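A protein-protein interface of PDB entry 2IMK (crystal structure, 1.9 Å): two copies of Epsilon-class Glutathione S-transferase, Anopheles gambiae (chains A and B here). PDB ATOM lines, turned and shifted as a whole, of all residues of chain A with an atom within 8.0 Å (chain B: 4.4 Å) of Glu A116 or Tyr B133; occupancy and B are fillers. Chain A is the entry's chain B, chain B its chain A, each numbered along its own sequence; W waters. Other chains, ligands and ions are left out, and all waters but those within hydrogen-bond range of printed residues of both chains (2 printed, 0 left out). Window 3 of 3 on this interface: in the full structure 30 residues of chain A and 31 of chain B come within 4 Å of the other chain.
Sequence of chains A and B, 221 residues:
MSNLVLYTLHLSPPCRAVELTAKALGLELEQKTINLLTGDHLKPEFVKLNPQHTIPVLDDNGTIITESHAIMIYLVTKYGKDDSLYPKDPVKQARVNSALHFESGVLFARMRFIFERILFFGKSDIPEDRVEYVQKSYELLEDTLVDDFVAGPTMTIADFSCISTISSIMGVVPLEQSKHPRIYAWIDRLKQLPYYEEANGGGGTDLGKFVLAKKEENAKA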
ATOM      1  N   ALA A 109     -22.039  19.165  11.861  1.00  0.00           N
ATOM      2  CA  ALA A 109     -21.138  19.245  13.017  1.00  0.00           C
ATOM      3  C   ALA A 109     -20.193  18.045  13.184  1.00  0.00           C
ATOM      4  O   ALA A 109     -18.975  18.208  13.369  1.00  0.00           O
ATOM      5  CB  ALA A 109     -21.977  19.454  14.378  1.00  0.00           C
ATOM      6  N   ARG A 110     -20.742  16.844  13.124  1.00  0.00           N
ATOM      7  CA  ARG A 110     -19.942  15.659  13.294  1.00  0.00           C
ATOM      8  C   ARG A 110     -19.031  15.414  12.149  1.00  0.00           C
ATOM      9  O   ARG A 110     -17.860  15.067  12.374  1.00  0.00           O
ATOM     10  CB  ARG A 110     -20.817  14.466  13.676  1.00  0.00           C
ATOM     11  CG  ARG A 110     -21.504  14.765  15.143  1.00  0.00           C
ATOM     12  CD  ARG A 110     -22.470  13.643  15.441  1.00  0.00           C
ATOM     13  NE  ARG A 110     -23.224  13.881  16.666  1.00  0.00           N
ATOM     14  CZ  ARG A 110     -23.900  12.968  17.345  1.00  0.00           C
ATOM     15  NH1 ARG A 110     -23.919  11.672  16.950  1.00  0.00           N
ATOM     16  NH2 ARG A 110     -24.547  13.367  18.442  1.00  0.00           N
ATOM     17  N   MET A 111     -19.532  15.593  10.920  1.00  0.00           N
ATOM     18  CA  MET A 111     -18.668  15.630   9.733  1.00  0.00           C
ATOM     19  C   MET A 111     -17.501  16.649   9.878  1.00  0.00           C
ATOM     20  O   MET A 111     -16.335  16.307   9.663  1.00  0.00           O
ATOM     21  CB  MET A 111     -19.485  16.034   8.514  1.00  0.00           C
ATOM     22  CG  MET A 111     -18.725  15.834   7.238  1.00  0.00           C
ATOM     23  SD  MET A 111     -19.292  16.785   5.818  1.00  0.00           S
ATOM     24  CE  MET A 111     -18.516  18.352   6.300  1.00  0.00           C
ATOM     25  N   ARG A 112     -17.818  17.910  10.207  1.00  0.00           N
ATOM     26  CA  ARG A 112     -16.805  18.910  10.405  1.00  0.00           C
ATOM     27  C   ARG A 112     -15.788  18.482  11.502  1.00  0.00           C
ATOM     28  O   ARG A 112     -14.573  18.651  11.299  1.00  0.00           O
ATOM     29  CB  ARG A 112     -17.434  20.229  10.753  1.00  0.00           C
ATOM     30  CG  ARG A 112     -16.533  21.386  10.356  1.00  0.00           C
ATOM     31  CD  ARG A 112     -17.095  22.758  10.836  1.00  0.00           C
ATOM     32  NE  ARG A 112     -15.984  23.628  11.268  1.00  0.00           N
ATOM     33  CZ  ARG A 112     -15.811  24.897  10.892  1.00  0.00           C
ATOM     34  NH1 ARG A 112     -14.748  25.580  11.304  1.00  0.00           N
ATOM     35  NH2 ARG A 112     -16.711  25.499  10.135  1.00  0.00           N
ATOM     36  N   PHE A 113     -16.265  17.892  12.612  1.00  0.00           N
ATOM     37  CA  PHE A 113     -15.359  17.418  13.692  1.00  0.00           C
ATOM     38  C   PHE A 113     -14.347  16.403  13.180  1.00  0.00           C
ATOM     39  O   PHE A 113     -13.263  16.249  13.767  1.00  0.00           O
ATOM     40  CB  PHE A 113     -16.102  16.731  14.838  1.00  0.00           C
ATOM     41  CG  PHE A 113     -16.850  17.649  15.753  1.00  0.00           C
ATOM     42  CD1 PHE A 113     -17.920  17.133  16.543  1.00  0.00           C
ATOM     43  CD2 PHE A 113     -16.564  19.000  15.817  1.00  0.00           C
ATOM     44  CE1 PHE A 113     -18.681  17.972  17.418  1.00  0.00           C
ATOM     45  CE2 PHE A 113     -17.337  19.879  16.696  1.00  0.00           C
ATOM     46  CZ  PHE A 113     -18.376  19.345  17.500  1.00  0.00           C
ATOM     47  N   ILE A 114     -14.723  15.678  12.129  1.00  0.00           N
ATOM     48  CA  ILE A 114     -13.833  14.735  11.419  1.00  0.00           C
ATOM     49  C   ILE A 114     -12.961  15.337  10.311  1.00  0.00           C
ATOM     50  O   ILE A 114     -11.763  14.993  10.219  1.00  0.00           O
ATOM     51  CB  ILE A 114     -14.663  13.595  10.832  1.00  0.00           C
ATOM     52  CG1 ILE A 114     -15.399  12.998  11.984  1.00  0.00           C
ATOM     53  CG2 ILE A 114     -13.802  12.438  10.272  1.00  0.00           C
ATOM     54  CD1 ILE A 114     -16.580  12.446  11.584  1.00  0.00           C
ATOM     55  N   PHE A 115     -13.534  16.222   9.482  1.00  0.00           N
ATOM     56  CA  PHE A 115     -12.840  16.714   8.290  1.00  0.00           C
ATOM     57  C   PHE A 115     -11.872  17.839   8.629  1.00  0.00           C
ATOM     58  O   PHE A 115     -10.799  17.912   8.030  1.00  0.00           O
ATOM     59  CB  PHE A 115     -13.843  17.198   7.201  1.00  0.00           C
ATOM     60  CG  PHE A 115     -14.535  16.069   6.421  1.00  0.00           C
ATOM     61  CD1 PHE A 115     -14.390  14.730   6.797  1.00  0.00           C
ATOM     62  CD2 PHE A 115     -15.358  16.375   5.316  1.00  0.00           C
ATOM     63  CE1 PHE A 115     -15.007  13.685   6.076  1.00  0.00           C
ATOM     64  CE2 PHE A 115     -15.994  15.358   4.568  1.00  0.00           C
ATOM     65  CZ  PHE A 115     -15.824  13.992   4.945  1.00  0.00           C
ATOM     66  N   GLU A 116     -12.240  18.727   9.562  1.00  0.00           N
ATOM     67  CA  GLU A 116     -11.538  20.024   9.721  1.00  0.00           C
ATOM     68  C   GLU A 116     -10.115  19.820  10.238  1.00  0.00           C
ATOM     69  O   GLU A 116      -9.157  20.361   9.669  1.00  0.00           O
ATOM     70  CB  GLU A 116     -12.300  20.943  10.639  1.00  0.00           C
ATOM     71  CG  GLU A 116     -11.675  22.323  10.821  1.00  0.00           C
ATOM     72  CD  GLU A 116     -12.413  23.167  11.839  1.00  0.00           C
ATOM     73  OE1 GLU A 116     -13.459  22.774  12.402  1.00  0.00           O
ATOM     74  OE2 GLU A 116     -11.937  24.278  12.088  1.00  0.00           O
ATOM     75  N   ARG A 117      -9.977  19.014  11.280  1.00  0.00           N
ATOM     76  CA  ARG A 117      -8.662  18.676  11.778  1.00  0.00           C
ATOM     77  C   ARG A 117      -7.706  18.102  10.679  1.00  0.00           C
ATOM     78  O   ARG A 117      -6.502  18.268  10.809  1.00  0.00           O
ATOM     79  CB  ARG A 117      -8.772  17.769  13.025  1.00  0.00           C
ATOM     80  CG  ARG A 117      -9.425  16.418  12.762  1.00  0.00           C
ATOM     81  CD  ARG A 117      -9.708  15.624  14.018  1.00  0.00           C
ATOM     82  NE  ARG A 117      -8.519  15.197  14.765  1.00  0.00           N
ATOM     83  CZ  ARG A 117      -7.704  14.190  14.440  1.00  0.00           C
ATOM     84  NH1 ARG A 117      -7.905  13.445  13.365  1.00  0.00           N
ATOM     85  NH2 ARG A 117      -6.648  13.930  15.201  1.00  0.00           N
ATOM     86  N   ILE A 118      -8.235  17.441   9.638  1.00  0.00           N
ATOM     87  CA  ILE A 118      -7.449  16.944   8.501  1.00  0.00           C
ATOM     88  C   ILE A 118      -7.173  18.031   7.420  1.00  0.00           C
ATOM     89  O   ILE A 118      -6.020  18.203   6.965  1.00  0.00           O
ATOM     90  CB  ILE A 118      -8.086  15.658   7.842  1.00  0.00           C
ATOM     91  CG1 ILE A 118      -7.983  14.456   8.765  1.00  0.00           C
ATOM     92  CG2 ILE A 118      -7.476  15.327   6.465  1.00  0.00           C
ATOM     93  CD1 ILE A 118      -9.043  13.448   8.467  1.00  0.00           C
ATOM     94  N   LEU A 119      -8.215  18.745   7.004  1.00  0.00           N
ATOM     95  CA  LEU A 119      -8.104  19.716   5.922  1.00  0.00           C
ATOM     96  C   LEU A 119      -7.349  20.995   6.335  1.00  0.00           C
ATOM     97  O   LEU A 119      -6.664  21.635   5.529  1.00  0.00           O
ATOM     98  CB  LEU A 119      -9.494  20.061   5.429  1.00  0.00           C
ATOM     99  CG  LEU A 119     -10.346  18.931   4.826  1.00  0.00           C
ATOM    100  CD1 LEU A 119     -11.653  19.537   4.285  1.00  0.00           C
ATOM    101  CD2 LEU A 119      -9.608  18.102   3.717  1.00  0.00           C
ATOM    102  N   PHE A 120      -7.471  21.339   7.613  1.00  0.00           N
ATOM    103  CA  PHE A 120      -7.057  22.628   8.119  1.00  0.00           C
ATOM    104  C   PHE A 120      -6.021  22.589   9.260  1.00  0.00           C
ATOM    105  O   PHE A 120      -5.244  23.550   9.425  1.00  0.00           O
ATOM    106  CB  PHE A 120      -8.308  23.450   8.525  1.00  0.00           C
ATOM    107  CG  PHE A 120      -9.146  23.832   7.347  1.00  0.00           C
ATOM    108  CD1 PHE A 120      -8.721  24.854   6.475  1.00  0.00           C
ATOM    109  CD2 PHE A 120     -10.295  23.102   7.037  1.00  0.00           C
ATOM    110  CE1 PHE A 120      -9.452  25.183   5.339  1.00  0.00           C
ATOM    111  CE2 PHE A 120     -11.036  23.423   5.923  1.00  0.00           C
ATOM    112  CZ  PHE A 120     -10.604  24.484   5.058  1.00  0.00           C
ATOM    113  N   PHE A 121      -6.042  21.521  10.057  1.00  0.00           N
ATOM    114  CA  PHE A 121      -5.131  21.413  11.212  1.00  0.00           C
ATOM    115  C   PHE A 121      -3.984  20.390  10.988  1.00  0.00           C
ATOM    116  O   PHE A 121      -3.174  20.147  11.879  1.00  0.00           O
ATOM    117  CB  PHE A 121      -5.873  21.158  12.546  1.00  0.00           C
ATOM    118  CG  PHE A 121      -6.946  22.199  12.908  1.00  0.00           C
ATOM    119  CD1 PHE A 121      -8.093  21.801  13.618  1.00  0.00           C
ATOM    120  CD2 PHE A 121      -6.810  23.548  12.573  1.00  0.00           C
ATOM    121  CE1 PHE A 121      -9.080  22.710  13.974  1.00  0.00           C
ATOM    122  CE2 PHE A 121      -7.792  24.479  12.925  1.00  0.00           C
ATOM    123  CZ  PHE A 121      -8.933  24.062  13.615  1.00  0.00           C
ATOM    124  N   GLY A 122      -3.936  19.792   9.807  1.00  0.00           N
ATOM    125  CA  GLY A 122      -2.833  18.957   9.437  1.00  0.00           C
ATOM    126  C   GLY A 122      -2.745  17.576  10.028  1.00  0.00           C
ATOM    127  O   GLY A 122      -1.693  16.972   9.962  1.00  0.00           O
ATOM    128  N   LYS A 123      -3.835  17.040  10.556  1.00  0.00           N
ATOM    129  CA  LYS A 123      -3.828  15.690  11.142  1.00  0.00           C
ATOM    130  C   LYS A 123      -3.938  14.577  10.097  1.00  0.00           C
ATOM    131  O   LYS A 123      -4.430  14.798   8.987  1.00  0.00           O
ATOM    132  CB  LYS A 123      -4.963  15.552  12.135  1.00  0.00           C
ATOM    133  CG  LYS A 123      -4.917  16.571  13.262  1.00  0.00           C
ATOM    134  CD  LYS A 123      -3.684  16.350  14.145  1.00  0.00           C
ATOM    135  CE  LYS A 123      -3.737  17.259  15.332  1.00  0.00           C
ATOM    136  NZ  LYS A 123      -2.367  17.724  15.656  1.00  0.00           N
ATOM    137  N   ARG A 130     -14.607   9.757  16.889  1.00  0.00           N
ATOM    138  CA  ARG A 130     -15.098  10.424  15.674  1.00  0.00           C
ATOM    139  C   ARG A 130     -15.846   9.499  14.717  1.00  0.00           C
ATOM    140  O   ARG A 130     -16.835   9.920  14.131  1.00  0.00           O
ATOM    141  CB  ARG A 130     -13.933  11.055  14.892  1.00  0.00           C
ATOM    142  CG  ARG A 130     -13.047  11.970  15.706  1.00  0.00           C
ATOM    143  CD  ARG A 130     -13.795  13.217  16.066  1.00  0.00           C
ATOM    144  NE  ARG A 130     -12.961  14.428  16.125  1.00  0.00           N
ATOM    145  CZ  ARG A 130     -12.038  14.712  17.044  1.00  0.00           C
ATOM    146  NH1 ARG A 130     -11.724  13.850  17.992  1.00  0.00           N
ATOM    147  NH2 ARG A 130     -11.421  15.872  17.007  1.00  0.00           N
ATOM    148  N   VAL A 211     -10.393  14.505   1.261  1.00  0.00           N
ATOM    149  CA  VAL A 211     -10.066  14.384   2.676  1.00  0.00           C
ATOM    150  C   VAL A 211      -9.127  13.181   2.917  1.00  0.00           C
ATOM    151  O   VAL A 211      -8.137  13.295   3.654  1.00  0.00           O
ATOM    152  CB  VAL A 211     -11.358  14.273   3.539  1.00  0.00           C
ATOM    153  CG1 VAL A 211     -11.082  13.644   4.907  1.00  0.00           C
ATOM    154  CG2 VAL A 211     -12.017  15.659   3.682  1.00  0.00           C
ATOM    155  N   LYS A 214      -5.619  14.273   1.329  1.00  0.00           N
ATOM    156  CA  LYS A 214      -4.930  15.231   2.208  1.00  0.00           C
ATOM    157  C   LYS A 214      -4.470  14.594   3.551  1.00  0.00           C
ATOM    158  O   LYS A 214      -3.550  15.105   4.228  1.00  0.00           O
ATOM    159  CB  LYS A 214      -5.825  16.469   2.427  1.00  0.00           C
ATOM    160  CG  LYS A 214      -5.263  17.551   3.339  1.00  0.00           C
ATOM    161  CD  LYS A 214      -4.513  18.665   2.621  1.00  0.00           C
ATOM    162  CE  LYS A 214      -3.747  19.569   3.634  1.00  0.00           C
ATOM    163  NZ  LYS A 214      -2.766  20.565   3.011  1.00  0.00           N
ATOM    164  N   ASN A 218      -0.844  14.155   4.962  1.00  0.00           N
ATOM    165  CA  ASN A 218      -0.521  14.633   6.314  1.00  0.00           C
ATOM    166  C   ASN A 218       0.195  13.578   7.158  1.00  0.00           C
ATOM    167  O   ASN A 218       0.826  13.923   8.129  1.00  0.00           O
ATOM    168  CB  ASN A 218      -1.763  15.129   7.090  1.00  0.00           C
ATOM    169  CG  ASN A 218      -2.308  16.482   6.598  1.00  0.00           C
ATOM    170  OD1 ASN A 218      -1.603  17.280   5.989  1.00  0.00           O
ATOM    171  ND2 ASN A 218      -3.579  16.741   6.888  1.00  0.00           N
ATOM    172  N   ARG B 110     -20.492  21.979  19.979  1.00  0.00           N
ATOM    173  CA  ARG B 110     -19.170  21.979  20.581  1.00  0.00           C
ATOM    174  C   ARG B 110     -19.254  21.772  22.122  1.00  0.00           C
ATOM    175  O   ARG B 110     -18.412  21.109  22.686  1.00  0.00           O
ATOM    176  CB  ARG B 110     -18.438  23.237  20.167  1.00  0.00           C
ATOM    177  CG  ARG B 110     -17.965  23.169  18.714  1.00  0.00           C
ATOM    178  CD  ARG B 110     -17.529  24.483  18.250  1.00  0.00           C
ATOM    179  NE  ARG B 110     -17.418  24.564  16.787  1.00  0.00           N
ATOM    180  CZ  ARG B 110     -16.664  25.470  16.160  1.00  0.00           C
ATOM    181  NH1 ARG B 110     -15.897  26.311  16.877  1.00  0.00           N
ATOM    182  NH2 ARG B 110     -16.617  25.464  14.823  1.00  0.00           N
ATOM    183  N   ASP B 129      -8.218  19.951  22.088  1.00  0.00           N
ATOM    184  CA  ASP B 129      -8.949  20.385  20.883  1.00  0.00           C
ATOM    185  C   ASP B 129     -10.423  20.766  21.151  1.00  0.00           C
ATOM    186  O   ASP B 129     -10.951  21.724  20.574  1.00  0.00           O
ATOM    187  CB  ASP B 129      -8.876  19.300  19.771  1.00  0.00           C
ATOM    188  CG  ASP B 129      -9.450  17.918  20.206  1.00  0.00           C
ATOM    189  OD1 ASP B 129      -9.960  17.785  21.327  1.00  0.00           O
ATOM    190  OD2 ASP B 129      -9.376  16.929  19.431  1.00  0.00           O
ATOM    191  N   ARG B 130     -11.071  20.000  22.021  1.00  0.00           N
ATOM    192  CA  ARG B 130     -12.379  20.326  22.503  1.00  0.00           C
ATOM    193  C   ARG B 130     -12.388  21.721  23.151  1.00  0.00           C
ATOM    194  O   ARG B 130     -13.293  22.505  22.873  1.00  0.00           O
ATOM    195  CB  ARG B 130     -12.862  19.283  23.504  1.00  0.00           C
ATOM    196  CG  ARG B 130     -13.678  18.227  22.895  1.00  0.00           C
ATOM    197  CD  ARG B 130     -12.871  16.999  22.639  1.00  0.00           C
ATOM    198  NE  ARG B 130     -13.720  15.836  22.464  1.00  0.00           N
ATOM    199  CZ  ARG B 130     -13.358  14.792  21.758  1.00  0.00           C
ATOM    200  NH1 ARG B 130     -14.190  13.764  21.646  1.00  0.00           N
ATOM    201  NH2 ARG B 130     -12.142  14.781  21.185  1.00  0.00           N
ATOM    202  N   VAL B 131     -11.367  22.034  23.946  1.00  0.00           N
ATOM    203  CA  VAL B 131     -11.299  23.360  24.612  1.00  0.00           C
ATOM    204  C   VAL B 131     -11.160  24.416  23.536  1.00  0.00           C
ATOM    205  O   VAL B 131     -11.780  25.456  23.599  1.00  0.00           O
ATOM    206  CB  VAL B 131     -10.080  23.509  25.591  1.00  0.00           C
ATOM    207  CG1 VAL B 131     -10.121  24.875  26.303  1.00  0.00           C
ATOM    208  CG2 VAL B 131     -10.153  22.475  26.635  1.00  0.00           C
ATOM    209  N   GLU B 132     -10.328  24.131  22.534  1.00  0.00           N
ATOM    210  CA  GLU B 132     -10.052  25.057  21.413  1.00  0.00           C
ATOM    211  C   GLU B 132     -11.320  25.331  20.530  1.00  0.00           C
ATOM    212  O   GLU B 132     -11.638  26.481  20.252  1.00  0.00           O
ATOM    213  CB  GLU B 132      -8.868  24.522  20.581  1.00  0.00           C
ATOM    214  CG  GLU B 132      -7.520  24.775  21.276  1.00  0.00           C
ATOM    215  CD  GLU B 132      -6.315  23.959  20.745  1.00  0.00           C
ATOM    216  OE1 GLU B 132      -6.509  23.042  19.905  1.00  0.00           O
ATOM    217  OE2 GLU B 132      -5.148  24.252  21.206  1.00  0.00           O
ATOM    218  N   TYR B 133     -12.017  24.269  20.111  1.00  0.00           N
ATOM    219  CA  TYR B 133     -13.386  24.402  19.501  1.00  0.00           C
ATOM    220  C   TYR B 133     -14.263  25.349  20.298  1.00  0.00           C
ATOM    221  O   TYR B 133     -14.831  26.280  19.718  1.00  0.00           O
ATOM    222  CB  TYR B 133     -14.146  23.068  19.301  1.00  0.00           C
ATOM    223  CG  TYR B 133     -13.886  22.411  17.977  1.00  0.00           C
ATOM    224  CD1 TYR B 133     -14.125  23.079  16.777  1.00  0.00           C
ATOM    225  CD2 TYR B 133     -13.375  21.108  17.915  1.00  0.00           C
ATOM    226  CE1 TYR B 133     -13.923  22.452  15.526  1.00  0.00           C
ATOM    227  CE2 TYR B 133     -13.118  20.463  16.636  1.00  0.00           C
ATOM    228  CZ  TYR B 133     -13.403  21.165  15.465  1.00  0.00           C
ATOM    229  OH  TYR B 133     -13.148  20.576  14.240  1.00  0.00           O
ATOM    230  N   VAL B 134     -14.404  25.095  21.591  1.00  0.00           N
ATOM    231  CA  VAL B 134     -15.206  25.951  22.465  1.00  0.00           C
ATOM    232  C   VAL B 134     -14.750  27.428  22.487  1.00  0.00           C
ATOM    233  O   VAL B 134     -15.553  28.302  22.175  1.00  0.00           O
ATOM    234  CB  VAL B 134     -15.354  25.411  23.879  1.00  0.00           C
ATOM    235  CG1 VAL B 134     -16.075  26.428  24.778  1.00  0.00           C
ATOM    236  CG2 VAL B 134     -16.134  24.076  23.876  1.00  0.00           C
ATOM    237  N   GLN B 135     -13.492  27.701  22.853  1.00  0.00           N
ATOM    238  CA  GLN B 135     -12.948  29.038  22.803  1.00  0.00           C
ATOM    239  C   GLN B 135     -13.208  29.706  21.470  1.00  0.00           C
ATOM    240  O   GLN B 135     -13.598  30.876  21.393  1.00  0.00           O
ATOM    241  CB  GLN B 135     -11.416  29.031  23.116  1.00  0.00           C
ATOM    242  CG  GLN B 135     -11.074  28.656  24.597  1.00  0.00           C
ATOM    243  CD  GLN B 135     -11.557  29.733  25.606  1.00  0.00           C
ATOM    244  OE1 GLN B 135     -11.601  29.481  26.820  1.00  0.00           O
ATOM    245  NE2 GLN B 135     -11.854  30.956  25.109  1.00  0.00           N
ATOM    246  N   LYS B 136     -13.016  28.965  20.383  1.00  0.00           N
ATOM    247  CA  LYS B 136     -13.332  29.488  19.071  1.00  0.00           C
ATOM    248  C   LYS B 136     -14.852  29.833  18.886  1.00  0.00           C
ATOM    249  O   LYS B 136     -15.197  30.856  18.282  1.00  0.00           O
ATOM    250  CB  LYS B 136     -12.727  28.578  17.982  1.00  0.00           C
ATOM    251  CG  LYS B 136     -12.920  29.159  16.589  1.00  0.00           C
ATOM    252  CD  LYS B 136     -11.728  30.023  16.050  1.00  0.00           C
ATOM    253  CE  LYS B 136     -12.091  30.755  14.735  1.00  0.00           C
ATOM    254  NZ  LYS B 136     -12.961  32.009  14.927  1.00  0.00           N
ATOM    255  N   SER B 137     -15.732  29.052  19.486  1.00  0.00           N
ATOM    256  CA  SER B 137     -17.157  29.336  19.420  1.00  0.00           C
ATOM    257  C   SER B 137     -17.405  30.693  20.137  1.00  0.00           C
ATOM    258  O   SER B 137     -18.216  31.475  19.670  1.00  0.00           O
ATOM    259  CB  SER B 137     -17.983  28.223  20.071  1.00  0.00           C
ATOM    260  OG  SER B 137     -18.052  28.326  21.519  1.00  0.00           O
HETATM  261  O   HOH W   1     -18.388  24.425  12.898  1.00  0.00           O
HETATM  262  O   HOH W   2     -11.892  18.536  13.212  1.00  0.00           O
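Ile A114 touches none of the printed residues of chain B.
Of chain B, only Tyr B133 (2.9 Å) comes within 4 Å of Glu A116.
Of the printed residues of chain A, Asp B129 touches Arg A130.
Of the printed residues of chain A, Arg B130 touches Arg A130 (3.4 Å).
Lys B136 touches none of the printed residues of chain A.
The nearest printed residue of chain B that does not touch Glu A116 is Arg B110 (4.8 Å).
The nearest printed residue of chain A that does not touch Tyr B133 is Phe A121 (4.6 Å).
The nearest printed residue of chain B that does not touch Phe A113 is Asp B129 (6.9 Å).
Arg B130 touches its own counterpart, Arg A130.
2 positions are printed for both chains.
Of the 7 pairs that touch across the chains among the printed residues, 1 has its exchanged pair printed and touching as well.
OD2 of Asp B129 is in salt-bridge range of NH2 of Arg A130, 3.3 Å away.
The side-chain hydroxyl (OH) of Tyr B133 lies within hydrogen-bond range of the side-chain carboxylate (OE1) of Glu A116, at 2.9 Å.
NH1 of Arg A130 sits close to NH2 of Arg B130 (3.4 Å).
Water W2 lies within hydrogen-bond range of OH of Tyr B133, O of Phe A113, N of Arg A117 and O of Arg A112.
Water W1 lies within hydrogen-bond range of NH2 of Arg B110 (2.8 Å) and NE of Arg A112 (3.0 Å).
Among the printed residues, merely in contact across the chains: Arg A112 with Arg B110 (3.99 Å), Arg A112 with Tyr B133 (3.8 Å), Phe A113 with Arg B110 (3.9 Å) and Phe A113 with Tyr B133 (3.8 Å).
The guanidinium group (NH1) of Arg B110 lies within hydrogen-bond range of the backbone carbonyl oxygen (O) of Tyr B133, 3.0 Å away.
The guanidinium group of Arg B130 is in salt-bridge range of the side-chain carboxylate of Asp B129 (3.7 Å).
NE of Arg A112 is in salt-bridge range of OE1 of Glu A116 (2.9 Å).
The backbone carbonyl oxygen (O) of Phe A113 lies within hydrogen-bond range of the guanidinium group (NE) of Arg A130, at 3.0 Å.
The backbone NH (N) of Phe A121 sits at hydrogen-bond distance from the backbone carbonyl oxygen (O) of Glu A116.
Hydrophobic or aromatic side chains of chain A that line the printed part of chain B: Phe A113.
Among the printed residues, 7 pairs touch across the chains.
Among the printed residues, Asp or Glu carboxylates within 4 Å of a Lys or Arg side-chain nitrogen of the other chain: Arg A130 with Asp B129 (3.3 Å).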
